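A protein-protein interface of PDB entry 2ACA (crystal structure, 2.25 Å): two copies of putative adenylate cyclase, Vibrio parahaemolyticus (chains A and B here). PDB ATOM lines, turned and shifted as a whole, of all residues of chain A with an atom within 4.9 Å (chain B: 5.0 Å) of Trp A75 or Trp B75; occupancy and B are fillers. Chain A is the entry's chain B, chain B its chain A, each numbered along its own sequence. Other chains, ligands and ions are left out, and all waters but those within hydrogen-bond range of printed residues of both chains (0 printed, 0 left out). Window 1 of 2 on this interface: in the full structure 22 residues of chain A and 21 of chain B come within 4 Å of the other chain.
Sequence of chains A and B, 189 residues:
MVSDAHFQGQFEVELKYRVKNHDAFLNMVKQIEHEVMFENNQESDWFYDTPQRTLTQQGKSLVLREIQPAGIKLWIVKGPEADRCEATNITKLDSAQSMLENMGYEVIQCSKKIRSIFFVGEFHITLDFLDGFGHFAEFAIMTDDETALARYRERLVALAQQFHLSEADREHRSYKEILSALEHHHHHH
SD of Met A99 lies close to O of Glu B86 (3.5 Å).
The side-chain sulfur (SD) of Met A99 sits close to the backbone carbonyl oxygen (O) of Trp B75.
The backbone carbonyl oxygen (O) of Glu A86 lies close to the side-chain sulfur (SD) of Met B99 (3.6 Å).
The side-chain sulfur of Met B99 sits close to the backbone carbonyl oxygen of Trp A75, 3.6 Å away.
N of Trp A75 lies within hydrogen-bond range of O of Thr A88, at 3.0 Å.
The backbone carbonyl oxygen of Val B77 sits at hydrogen-bond distance from the backbone NH of Glu B86 (2.9 Å).
The backbone NH (N) of Ile B90 is in hydrogen-bond range of the backbone carbonyl oxygen (O) of Lys B73 (3.0 Å).
N of Trp B75 is in hydrogen-bond range of O of Thr B88 (3.1 Å).
The backbone NH (N) of Glu A86 sits at hydrogen-bond distance from the backbone carbonyl oxygen (O) of Val A77 (3.0 Å).
The backbone carbonyl oxygen (O) of Lys A73 sits at hydrogen-bond distance from the backbone NH (N) of Ile A90, 2.9 Å away.
Among the printed residues, merely in contact across the chains: Met A99 with Thr B88, Trp A75 with Trp B75, Thr A88 with Met B99, Leu A62 with Met B103, Ala A96 with Trp B75, Met A99 with Ala B87, Thr A88 with Ile B90, Ile A90 with Thr B88, Met A99 with Val B77, Val A77 with Met B99, Trp A75 with Ala B96, Met A103 with Leu B62, Ala A87 with Met B99, Leu A100 with Met B103, Leu A100 with Trp B75 and Trp A75 with Met B103.
Of the printed residues of chain B, Trp A75 touches Trp B75 (3.5 Å), Ala B96 (3.8 Å), Met B99 (3.6 Å) and Met B103 (3.9 Å).
Trp B75 touches just these residues of chain A: Trp A75 (3.5 Å), Ala A96 (3.6 Å), Met A99 (3.6 Å) and Leu A100 (3.9 Å).
Printed residues of chain B within 4 Å of Val A77: Met B99 (3.8 Å).
Of the printed residues of chain A, Leu B62 touches Met A103 (3.8 Å).
Lys A73 touches none of the printed residues of chain B.
Ile A76 touches none of the printed residues of chain B.
The nearest printed residue of chain B that does not touch Trp A75 is Leu B100 (4.003 Å).
The nearest residue of chain A that does not touch Trp B75 is Met A103 (4.05 Å).
The nearest printed residue of chain B that does not touch Ala A87 is Ala B96 (5.8 Å).
Of the 16 printed residues of chain B, 10 touch a printed residue of chain A.
Hydrophobic or aromatic side chains of chain A that line the printed part of chain B: Leu A62, Trp A75, Val A77, Ile A90, Ala A96, Met A99, Leu A100 and Met A103.
Among the printed residues, 20 pairs touch across the chains.
Leu A62 touches Met B103, and with the chains exchanged Met A103 touches Leu B62.
Trp A75 touches Ala B96, and with the chains exchanged Ala A96 touches Trp B75.
Trp A75 touches Met B103, but with the chains exchanged Met A103 does not touch Trp B75 (4.05 Å).
Leu A100 touches Trp B75, but with the chains exchanged Trp A75 does not touch Leu B100 (4.003 Å).
16 positions are printed for both chains.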
ATOM      1  N   LEU A  62     -15.873  28.368  -6.637  1.00  0.00           N
ATOM      2  CA  LEU A  62     -14.417  28.413  -6.571  1.00  0.00           C
ATOM      3  C   LEU A  62     -14.135  29.037  -5.211  1.00  0.00           C
ATOM      4  O   LEU A  62     -14.430  30.210  -4.986  1.00  0.00           O
ATOM      5  CB  LEU A  62     -13.871  29.272  -7.706  1.00  0.00           C
ATOM      6  CG  LEU A  62     -12.450  29.822  -7.573  1.00  0.00           C
ATOM      7  CD1 LEU A  62     -11.479  28.714  -7.247  1.00  0.00           C
ATOM      8  CD2 LEU A  62     -12.077  30.534  -8.875  1.00  0.00           C
ATOM      9  N   VAL A  63     -13.560  28.249  -4.315  1.00  0.00           N
ATOM     10  CA  VAL A  63     -13.314  28.699  -2.954  1.00  0.00           C
ATOM     11  C   VAL A  63     -11.891  28.589  -2.386  1.00  0.00           C
ATOM     12  O   VAL A  63     -11.179  27.625  -2.655  1.00  0.00           O
ATOM     13  CB  VAL A  63     -14.232  27.910  -1.975  1.00  0.00           C
ATOM     14  CG1 VAL A  63     -14.099  28.465  -0.569  1.00  0.00           C
ATOM     15  CG2 VAL A  63     -15.679  27.964  -2.444  1.00  0.00           C
ATOM     16  N   LEU A  64     -11.507  29.589  -1.589  1.00  0.00           N
ATOM     17  CA  LEU A  64     -10.228  29.584  -0.866  1.00  0.00           C
ATOM     18  C   LEU A  64     -10.688  29.494   0.593  1.00  0.00           C
ATOM     19  O   LEU A  64     -11.467  30.324   1.058  1.00  0.00           O
ATOM     20  CB  LEU A  64      -9.420  30.872  -1.092  1.00  0.00           C
ATOM     21  CG  LEU A  64      -8.787  31.007  -2.478  1.00  0.00           C
ATOM     22  CD1 LEU A  64      -7.776  32.154  -2.481  1.00  0.00           C
ATOM     23  CD2 LEU A  64      -8.096  29.682  -2.845  1.00  0.00           C
ATOM     24  N   LYS A  73      -5.347  25.144   5.036  1.00  0.00           N
ATOM     25  CA  LYS A  73      -5.645  26.085   3.970  1.00  0.00           C
ATOM     26  C   LYS A  73      -5.933  25.337   2.666  1.00  0.00           C
ATOM     27  O   LYS A  73      -5.120  24.533   2.191  1.00  0.00           O
ATOM     28  CB  LYS A  73      -4.486  27.062   3.811  1.00  0.00           C
ATOM     29  CG  LYS A  73      -4.444  28.086   4.928  1.00  0.00           C
ATOM     30  CD  LYS A  73      -3.142  28.859   4.963  1.00  0.00           C
ATOM     31  CE  LYS A  73      -2.058  28.076   5.672  1.00  0.00           C
ATOM     32  NZ  LYS A  73      -0.860  28.932   5.885  1.00  0.00           N
ATOM     33  N   LEU A  74      -7.089  25.628   2.082  1.00  0.00           N
ATOM     34  CA  LEU A  74      -7.513  24.932   0.880  1.00  0.00           C
ATOM     35  C   LEU A  74      -7.976  25.784  -0.280  1.00  0.00           C
ATOM     36  O   LEU A  74      -8.474  26.897  -0.110  1.00  0.00           O
ATOM     37  CB  LEU A  74      -8.644  23.948   1.233  1.00  0.00           C
ATOM     38  CG  LEU A  74      -8.351  22.889   2.299  1.00  0.00           C
ATOM     39  CD1 LEU A  74      -9.665  22.361   2.873  1.00  0.00           C
ATOM     40  CD2 LEU A  74      -7.527  21.742   1.692  1.00  0.00           C
ATOM     41  N   TRP A  75      -7.782  25.231  -1.471  1.00  0.00           N
ATOM     42  CA  TRP A  75      -8.225  25.839  -2.715  1.00  0.00           C
ATOM     43  C   TRP A  75      -9.256  24.803  -3.168  1.00  0.00           C
ATOM     44  O   TRP A  75      -8.918  23.630  -3.366  1.00  0.00           O
ATOM     45  CB  TRP A  75      -7.060  25.949  -3.693  1.00  0.00           C
ATOM     46  CG  TRP A  75      -7.428  26.123  -5.125  1.00  0.00           C
ATOM     47  CD1 TRP A  75      -8.613  26.570  -5.627  1.00  0.00           C
ATOM     48  CD2 TRP A  75      -6.587  25.862  -6.252  1.00  0.00           C
ATOM     49  NE1 TRP A  75      -8.569  26.604  -6.998  1.00  0.00           N
ATOM     50  CE2 TRP A  75      -7.334  26.173  -7.410  1.00  0.00           C
ATOM     51  CE3 TRP A  75      -5.271  25.392  -6.396  1.00  0.00           C
ATOM     52  CZ2 TRP A  75      -6.812  26.025  -8.708  1.00  0.00           C
ATOM     53  CZ3 TRP A  75      -4.753  25.240  -7.681  1.00  0.00           C
ATOM     54  CH2 TRP A  75      -5.526  25.557  -8.821  1.00  0.00           C
ATOM     55  N   ILE A  76     -10.507  25.234  -3.318  1.00  0.00           N
ATOM     56  CA  ILE A  76     -11.591  24.318  -3.668  1.00  0.00           C
ATOM     57  C   ILE A  76     -12.483  24.708  -4.842  1.00  0.00           C
ATOM     58  O   ILE A  76     -12.755  25.889  -5.077  1.00  0.00           O
ATOM     59  CB  ILE A  76     -12.543  24.122  -2.440  1.00  0.00           C
ATOM     60  CG1 ILE A  76     -11.763  23.609  -1.233  1.00  0.00           C
ATOM     61  CG2 ILE A  76     -13.661  23.130  -2.768  1.00  0.00           C
ATOM     62  CD1 ILE A  76     -12.514  23.793   0.084  1.00  0.00           C
ATOM     63  N   VAL A  77     -12.935  23.690  -5.572  1.00  0.00           N
ATOM     64  CA  VAL A  77     -13.890  23.876  -6.660  1.00  0.00           C
ATOM     65  C   VAL A  77     -14.949  22.785  -6.524  1.00  0.00           C
ATOM     66  O   VAL A  77     -14.637  21.596  -6.568  1.00  0.00           O
ATOM     67  CB  VAL A  77     -13.260  23.769  -8.056  1.00  0.00           C
ATOM     68  CG1 VAL A  77     -14.362  23.808  -9.109  1.00  0.00           C
ATOM     69  CG2 VAL A  77     -12.300  24.934  -8.291  1.00  0.00           C
ATOM     70  N   GLU A  86     -13.591  19.010  -5.582  1.00  0.00           N
ATOM     71  CA  GLU A  86     -12.155  18.791  -5.671  1.00  0.00           C
ATOM     72  C   GLU A  86     -11.418  19.848  -4.855  1.00  0.00           C
ATOM     73  O   GLU A  86     -11.894  20.974  -4.714  1.00  0.00           O
ATOM     74  CB  GLU A  86     -11.698  18.850  -7.130  1.00  0.00           C
ATOM     75  CG  GLU A  86     -12.410  17.857  -8.041  1.00  0.00           C
ATOM     76  CD  GLU A  86     -11.688  17.658  -9.364  1.00  0.00           C
ATOM     77  OE1 GLU A  86     -10.577  17.083  -9.352  1.00  0.00           O
ATOM     78  OE2 GLU A  86     -12.224  18.078 -10.411  1.00  0.00           O
ATOM     79  N   ALA A  87     -10.253  19.488  -4.329  1.00  0.00           N
ATOM     80  CA  ALA A  87      -9.476  20.417  -3.524  1.00  0.00           C
ATOM     81  C   ALA A  87      -8.021  20.007  -3.337  1.00  0.00           C
ATOM     82  O   ALA A  87      -7.643  18.857  -3.556  1.00  0.00           O
ATOM     83  CB  ALA A  87     -10.128  20.568  -2.151  1.00  0.00           C
ATOM     84  N   THR A  88      -7.213  20.977  -2.926  1.00  0.00           N
ATOM     85  CA  THR A  88      -5.805  20.741  -2.631  1.00  0.00           C
ATOM     86  C   THR A  88      -5.399  21.738  -1.563  1.00  0.00           C
ATOM     87  O   THR A  88      -5.852  22.873  -1.581  1.00  0.00           O
ATOM     88  CB  THR A  88      -4.883  20.959  -3.863  1.00  0.00           C
ATOM     89  OG1 THR A  88      -3.521  20.742  -3.475  1.00  0.00           O
ATOM     90  CG2 THR A  88      -5.003  22.386  -4.400  1.00  0.00           C
ATOM     91  N   ILE A  90      -3.010  24.363   0.220  1.00  0.00           N
ATOM     92  CA  ILE A  90      -2.083  25.373  -0.275  1.00  0.00           C
ATOM     93  C   ILE A  90      -1.355  25.915   0.960  1.00  0.00           C
ATOM     94  O   ILE A  90      -1.909  25.926   2.062  1.00  0.00           O
ATOM     95  CB  ILE A  90      -2.811  26.545  -0.991  1.00  0.00           C
ATOM     96  CG1 ILE A  90      -3.888  27.132  -0.070  1.00  0.00           C
ATOM     97  CG2 ILE A  90      -3.409  26.065  -2.327  1.00  0.00           C
ATOM     98  CD1 ILE A  90      -4.651  28.301  -0.670  1.00  0.00           C
ATOM     99  N   ALA A  96      -2.523  32.778  -3.153  1.00  0.00           N
ATOM    100  CA  ALA A  96      -3.647  32.219  -3.901  1.00  0.00           C
ATOM    101  C   ALA A  96      -4.671  33.323  -4.140  1.00  0.00           C
ATOM    102  O   ALA A  96      -5.186  33.481  -5.247  1.00  0.00           O
ATOM    103  CB  ALA A  96      -4.282  31.072  -3.117  1.00  0.00           C
ATOM    104  N   MET A  99      -3.331  35.533  -6.787  1.00  0.00           N
ATOM    105  CA  MET A  99      -3.260  34.901  -8.101  1.00  0.00           C
ATOM    106  C   MET A  99      -4.647  34.830  -8.763  1.00  0.00           C
ATOM    107  O   MET A  99      -4.778  35.100  -9.955  1.00  0.00           O
ATOM    108  CB  MET A  99      -2.628  33.504  -7.993  1.00  0.00           C
ATOM    109  CG  MET A  99      -1.125  33.542  -7.734  1.00  0.00           C
ATOM    110  SD  MET A  99      -0.271  31.792  -7.775  1.00  0.00           S
ATOM    111  CE  MET A  99      -0.709  31.253  -5.973  1.00  0.00           C
ATOM    112  N   LEU A 100      -5.680  34.472  -8.003  1.00  0.00           N
ATOM    113  CA  LEU A 100      -7.037  34.419  -8.573  1.00  0.00           C
ATOM    114  C   LEU A 100      -7.450  35.808  -9.049  1.00  0.00           C
ATOM    115  O   LEU A 100      -8.165  35.962 -10.040  1.00  0.00           O
ATOM    116  CB  LEU A 100      -8.051  33.914  -7.541  1.00  0.00           C
ATOM    117  CG  LEU A 100      -7.942  32.438  -7.134  1.00  0.00           C
ATOM    118  CD1 LEU A 100      -9.128  32.059  -6.236  1.00  0.00           C
ATOM    119  CD2 LEU A 100      -7.920  31.569  -8.377  1.00  0.00           C
ATOM    120  N   MET A 103      -5.810  36.481 -12.219  1.00  0.00           N
ATOM    121  CA  MET A 103      -6.443  35.655 -13.242  1.00  0.00           C
ATOM    122  C   MET A 103      -7.831  36.147 -13.656  1.00  0.00           C
ATOM    123  O   MET A 103      -8.483  35.536 -14.503  1.00  0.00           O
ATOM    124  CB  MET A 103      -6.514  34.209 -12.756  1.00  0.00           C
ATOM    125  CG  MET A 103      -5.150  33.564 -12.613  1.00  0.00           C
ATOM    126  SD  MET A 103      -5.161  32.000 -11.502  1.00  0.00           S
ATOM    127  CE  MET A 103      -6.344  30.868 -12.538  1.00  0.00           C
ATOM    128  N   LEU B  62       0.313  31.132 -16.379  1.00  0.00           N
ATOM    129  CA  LEU B  62      -0.260  30.332 -15.302  1.00  0.00           C
ATOM    130  C   LEU B  62       0.410  28.973 -15.410  1.00  0.00           C
ATOM    131  O   LEU B  62       0.323  28.323 -16.443  1.00  0.00           O
ATOM    132  CB  LEU B  62      -1.771  30.206 -15.513  1.00  0.00           C
ATOM    133  CG  LEU B  62      -2.555  29.192 -14.678  1.00  0.00           C
ATOM    134  CD1 LEU B  62      -2.450  29.502 -13.197  1.00  0.00           C
ATOM    135  CD2 LEU B  62      -4.016  29.231 -15.125  1.00  0.00           C
ATOM    136  N   VAL B  63       1.073  28.540 -14.348  1.00  0.00           N
ATOM    137  CA  VAL B  63       1.788  27.279 -14.400  1.00  0.00           C
ATOM    138  C   VAL B  63       1.615  26.342 -13.215  1.00  0.00           C
ATOM    139  O   VAL B  63       1.564  26.777 -12.068  1.00  0.00           O
ATOM    140  CB  VAL B  63       3.323  27.557 -14.557  1.00  0.00           C
ATOM    141  CG1 VAL B  63       4.115  26.248 -14.545  1.00  0.00           C
ATOM    142  CG2 VAL B  63       3.587  28.342 -15.846  1.00  0.00           C
ATOM    143  N   LEU B  64       1.497  25.051 -13.503  1.00  0.00           N
ATOM    144  CA  LEU B  64       1.452  24.043 -12.464  1.00  0.00           C
ATOM    145  C   LEU B  64       2.837  23.412 -12.632  1.00  0.00           C
ATOM    146  O   LEU B  64       3.268  23.136 -13.763  1.00  0.00           O
ATOM    147  CB  LEU B  64       0.328  23.032 -12.708  1.00  0.00           C
ATOM    148  CG  LEU B  64      -1.076  23.553 -12.327  1.00  0.00           C
ATOM    149  CD1 LEU B  64      -2.114  22.445 -12.433  1.00  0.00           C
ATOM    150  CD2 LEU B  64      -1.042  24.087 -10.896  1.00  0.00           C
ATOM    151  N   LYS B  73       5.680  20.854  -5.431  1.00  0.00           N
ATOM    152  CA  LYS B  73       4.597  21.099  -6.379  1.00  0.00           C
ATOM    153  C   LYS B  73       4.089  22.515  -6.197  1.00  0.00           C
ATOM    154  O   LYS B  73       3.733  22.920  -5.088  1.00  0.00           O
ATOM    155  CB  LYS B  73       3.482  20.073  -6.148  1.00  0.00           C
ATOM    156  CG  LYS B  73       3.964  18.655  -6.413  1.00  0.00           C
ATOM    157  CD  LYS B  73       2.965  17.569  -6.043  1.00  0.00           C
ATOM    158  CE  LYS B  73       2.830  17.414  -4.543  1.00  0.00           C
ATOM    159  NZ  LYS B  73       2.176  16.116  -4.202  1.00  0.00           N
ATOM    160  N   LEU B  74       4.053  23.268  -7.285  1.00  0.00           N
ATOM    161  CA  LEU B  74       3.647  24.660  -7.201  1.00  0.00           C
ATOM    162  C   LEU B  74       2.593  25.099  -8.188  1.00  0.00           C
ATOM    163  O   LEU B  74       2.439  24.529  -9.254  1.00  0.00           O
ATOM    164  CB  LEU B  74       4.875  25.563  -7.384  1.00  0.00           C
ATOM    165  CG  LEU B  74       6.048  25.382  -6.409  1.00  0.00           C
ATOM    166  CD1 LEU B  74       7.358  25.691  -7.115  1.00  0.00           C
ATOM    167  CD2 LEU B  74       5.863  26.297  -5.200  1.00  0.00           C
ATOM    168  N   TRP B  75       1.869  26.134  -7.792  1.00  0.00           N
ATOM    169  CA  TRP B  75       0.857  26.763  -8.620  1.00  0.00           C
ATOM    170  C   TRP B  75       1.506  28.140  -8.789  1.00  0.00           C
ATOM    171  O   TRP B  75       1.781  28.826  -7.807  1.00  0.00           O
ATOM    172  CB  TRP B  75      -0.481  26.802  -7.859  1.00  0.00           C
ATOM    173  CG  TRP B  75      -1.486  27.770  -8.378  1.00  0.00           C
ATOM    174  CD1 TRP B  75      -1.537  28.323  -9.624  1.00  0.00           C
ATOM    175  CD2 TRP B  75      -2.595  28.303  -7.655  1.00  0.00           C
ATOM    176  NE1 TRP B  75      -2.609  29.173  -9.721  1.00  0.00           N
ATOM    177  CE2 TRP B  75      -3.279  29.178  -8.524  1.00  0.00           C
ATOM    178  CE3 TRP B  75      -3.083  28.123  -6.349  1.00  0.00           C
ATOM    179  CZ2 TRP B  75      -4.427  29.879  -8.135  1.00  0.00           C
ATOM    180  CZ3 TRP B  75      -4.220  28.819  -5.960  1.00  0.00           C
ATOM    181  CH2 TRP B  75      -4.882  29.688  -6.852  1.00  0.00           C
ATOM    182  N   ILE B  76       1.782  28.524 -10.033  1.00  0.00           N
ATOM    183  CA  ILE B  76       2.473  29.786 -10.317  1.00  0.00           C
ATOM    184  C   ILE B  76       1.813  30.719 -11.310  1.00  0.00           C
ATOM    185  O   ILE B  76       1.250  30.280 -12.311  1.00  0.00           O
ATOM    186  CB  ILE B  76       3.888  29.533 -10.931  1.00  0.00           C
ATOM    187  CG1 ILE B  76       4.625  28.432 -10.176  1.00  0.00           C
ATOM    188  CG2 ILE B  76       4.684  30.836 -10.989  1.00  0.00           C
ATOM    189  CD1 ILE B  76       4.791  28.675  -8.737  1.00  0.00           C
ATOM    190  N   VAL B  77       1.916  32.017 -11.043  1.00  0.00           N
ATOM    191  CA  VAL B  77       1.422  33.018 -11.978  1.00  0.00           C
ATOM    192  C   VAL B  77       2.475  34.124 -12.111  1.00  0.00           C
ATOM    193  O   VAL B  77       2.862  34.752 -11.121  1.00  0.00           O
ATOM    194  CB  VAL B  77       0.097  33.634 -11.540  1.00  0.00           C
ATOM    195  CG1 VAL B  77      -0.317  34.682 -12.539  1.00  0.00           C
ATOM    196  CG2 VAL B  77      -0.973  32.558 -11.454  1.00  0.00           C
ATOM    197  N   GLU B  86       4.051  35.229  -8.507  1.00  0.00           N
ATOM    198  CA  GLU B  86       3.410  34.743  -7.301  1.00  0.00           C
ATOM    199  C   GLU B  86       3.256  33.232  -7.368  1.00  0.00           C
ATOM    200  O   GLU B  86       3.101  32.653  -8.443  1.00  0.00           O
ATOM    201  CB  GLU B  86       2.055  35.424  -7.113  1.00  0.00           C
ATOM    202  CG  GLU B  86       2.164  36.938  -7.057  1.00  0.00           C
ATOM    203  CD  GLU B  86       0.869  37.610  -6.649  1.00  0.00           C
ATOM    204  OE1 GLU B  86       0.429  37.406  -5.497  1.00  0.00           O
ATOM    205  OE2 GLU B  86       0.293  38.340  -7.480  1.00  0.00           O
ATOM    206  N   ALA B  87       3.316  32.597  -6.211  1.00  0.00           N
ATOM    207  CA  ALA B  87       3.204  31.158  -6.151  1.00  0.00           C
ATOM    208  C   ALA B  87       2.773  30.690  -4.781  1.00  0.00           C
ATOM    209  O   ALA B  87       2.735  31.453  -3.824  1.00  0.00           O
ATOM    210  CB  ALA B  87       4.540  30.534  -6.480  1.00  0.00           C
ATOM    211  N   THR B  88       2.443  29.410  -4.711  1.00  0.00           N
ATOM    212  CA  THR B  88       2.090  28.779  -3.461  1.00  0.00           C
ATOM    213  C   THR B  88       2.261  27.298  -3.689  1.00  0.00           C
ATOM    214  O   THR B  88       1.993  26.800  -4.779  1.00  0.00           O
ATOM    215  CB  THR B  88       0.633  29.048  -3.038  1.00  0.00           C
ATOM    216  OG1 THR B  88       0.380  28.384  -1.795  1.00  0.00           O
ATOM    217  CG2 THR B  88      -0.341  28.519  -4.075  1.00  0.00           C
ATOM    218  N   ILE B  90       1.314  23.398  -3.387  1.00  0.00           N
ATOM    219  CA  ILE B  90       0.043  22.673  -3.400  1.00  0.00           C
ATOM    220  C   ILE B  90       0.389  21.222  -3.111  1.00  0.00           C
ATOM    221  O   ILE B  90       1.483  20.766  -3.456  1.00  0.00           O
ATOM    222  CB  ILE B  90      -0.678  22.776  -4.780  1.00  0.00           C
ATOM    223  CG1 ILE B  90       0.254  22.305  -5.904  1.00  0.00           C
ATOM    224  CG2 ILE B  90      -1.119  24.226  -5.043  1.00  0.00           C
ATOM    225  CD1 ILE B  90      -0.405  22.327  -7.289  1.00  0.00           C
ATOM    226  N   ALA B  96      -5.248  20.016  -8.694  1.00  0.00           N
ATOM    227  CA  ALA B  96      -5.014  21.352  -9.231  1.00  0.00           C
ATOM    228  C   ALA B  96      -5.252  21.389 -10.746  1.00  0.00           C
ATOM    229  O   ALA B  96      -5.901  22.303 -11.264  1.00  0.00           O
ATOM    230  CB  ALA B  96      -3.585  21.802  -8.909  1.00  0.00           C
ATOM    231  N   MET B  99      -9.000  21.060 -11.435  1.00  0.00           N
ATOM    232  CA  MET B  99      -9.734  22.272 -11.082  1.00  0.00           C
ATOM    233  C   MET B  99      -9.537  23.379 -12.114  1.00  0.00           C
ATOM    234  O   MET B  99     -10.487  24.077 -12.462  1.00  0.00           O
ATOM    235  CB  MET B  99      -9.322  22.770  -9.692  1.00  0.00           C
ATOM    236  CG  MET B  99      -9.873  21.942  -8.547  1.00  0.00           C
ATOM    237  SD  MET B  99      -9.453  22.672  -6.779  1.00  0.00           S
ATOM    238  CE  MET B  99      -7.672  21.936  -6.657  1.00  0.00           C
ATOM    239  N   LEU B 100      -8.311  23.547 -12.606  1.00  0.00           N
ATOM    240  CA  LEU B 100      -8.046  24.579 -13.610  1.00  0.00           C
ATOM    241  C   LEU B 100      -8.830  24.304 -14.905  1.00  0.00           C
ATOM    242  O   LEU B 100      -9.305  25.222 -15.572  1.00  0.00           O
ATOM    243  CB  LEU B 100      -6.543  24.669 -13.920  1.00  0.00           C
ATOM    244  CG  LEU B 100      -5.625  25.346 -12.898  1.00  0.00           C
ATOM    245  CD1 LEU B 100      -4.194  25.431 -13.450  1.00  0.00           C
ATOM    246  CD2 LEU B 100      -6.160  26.734 -12.594  1.00  0.00           C
ATOM    247  N   MET B 103     -12.185  25.195 -14.416  1.00  0.00           N
ATOM    248  CA  MET B 103     -12.249  26.658 -14.410  1.00  0.00           C
ATOM    249  C   MET B 103     -12.166  27.233 -15.820  1.00  0.00           C
ATOM    250  O   MET B 103     -12.090  28.447 -16.003  1.00  0.00           O
ATOM    251  CB  MET B 103     -11.131  27.235 -13.530  1.00  0.00           C
ATOM    252  CG  MET B 103     -11.440  27.153 -12.024  1.00  0.00           C
ATOM    253  SD  MET B 103      -9.893  27.117 -10.839  1.00  0.00           S
ATOM    254  CE  MET B 103      -9.453  29.002 -10.838  1.00  0.00           C
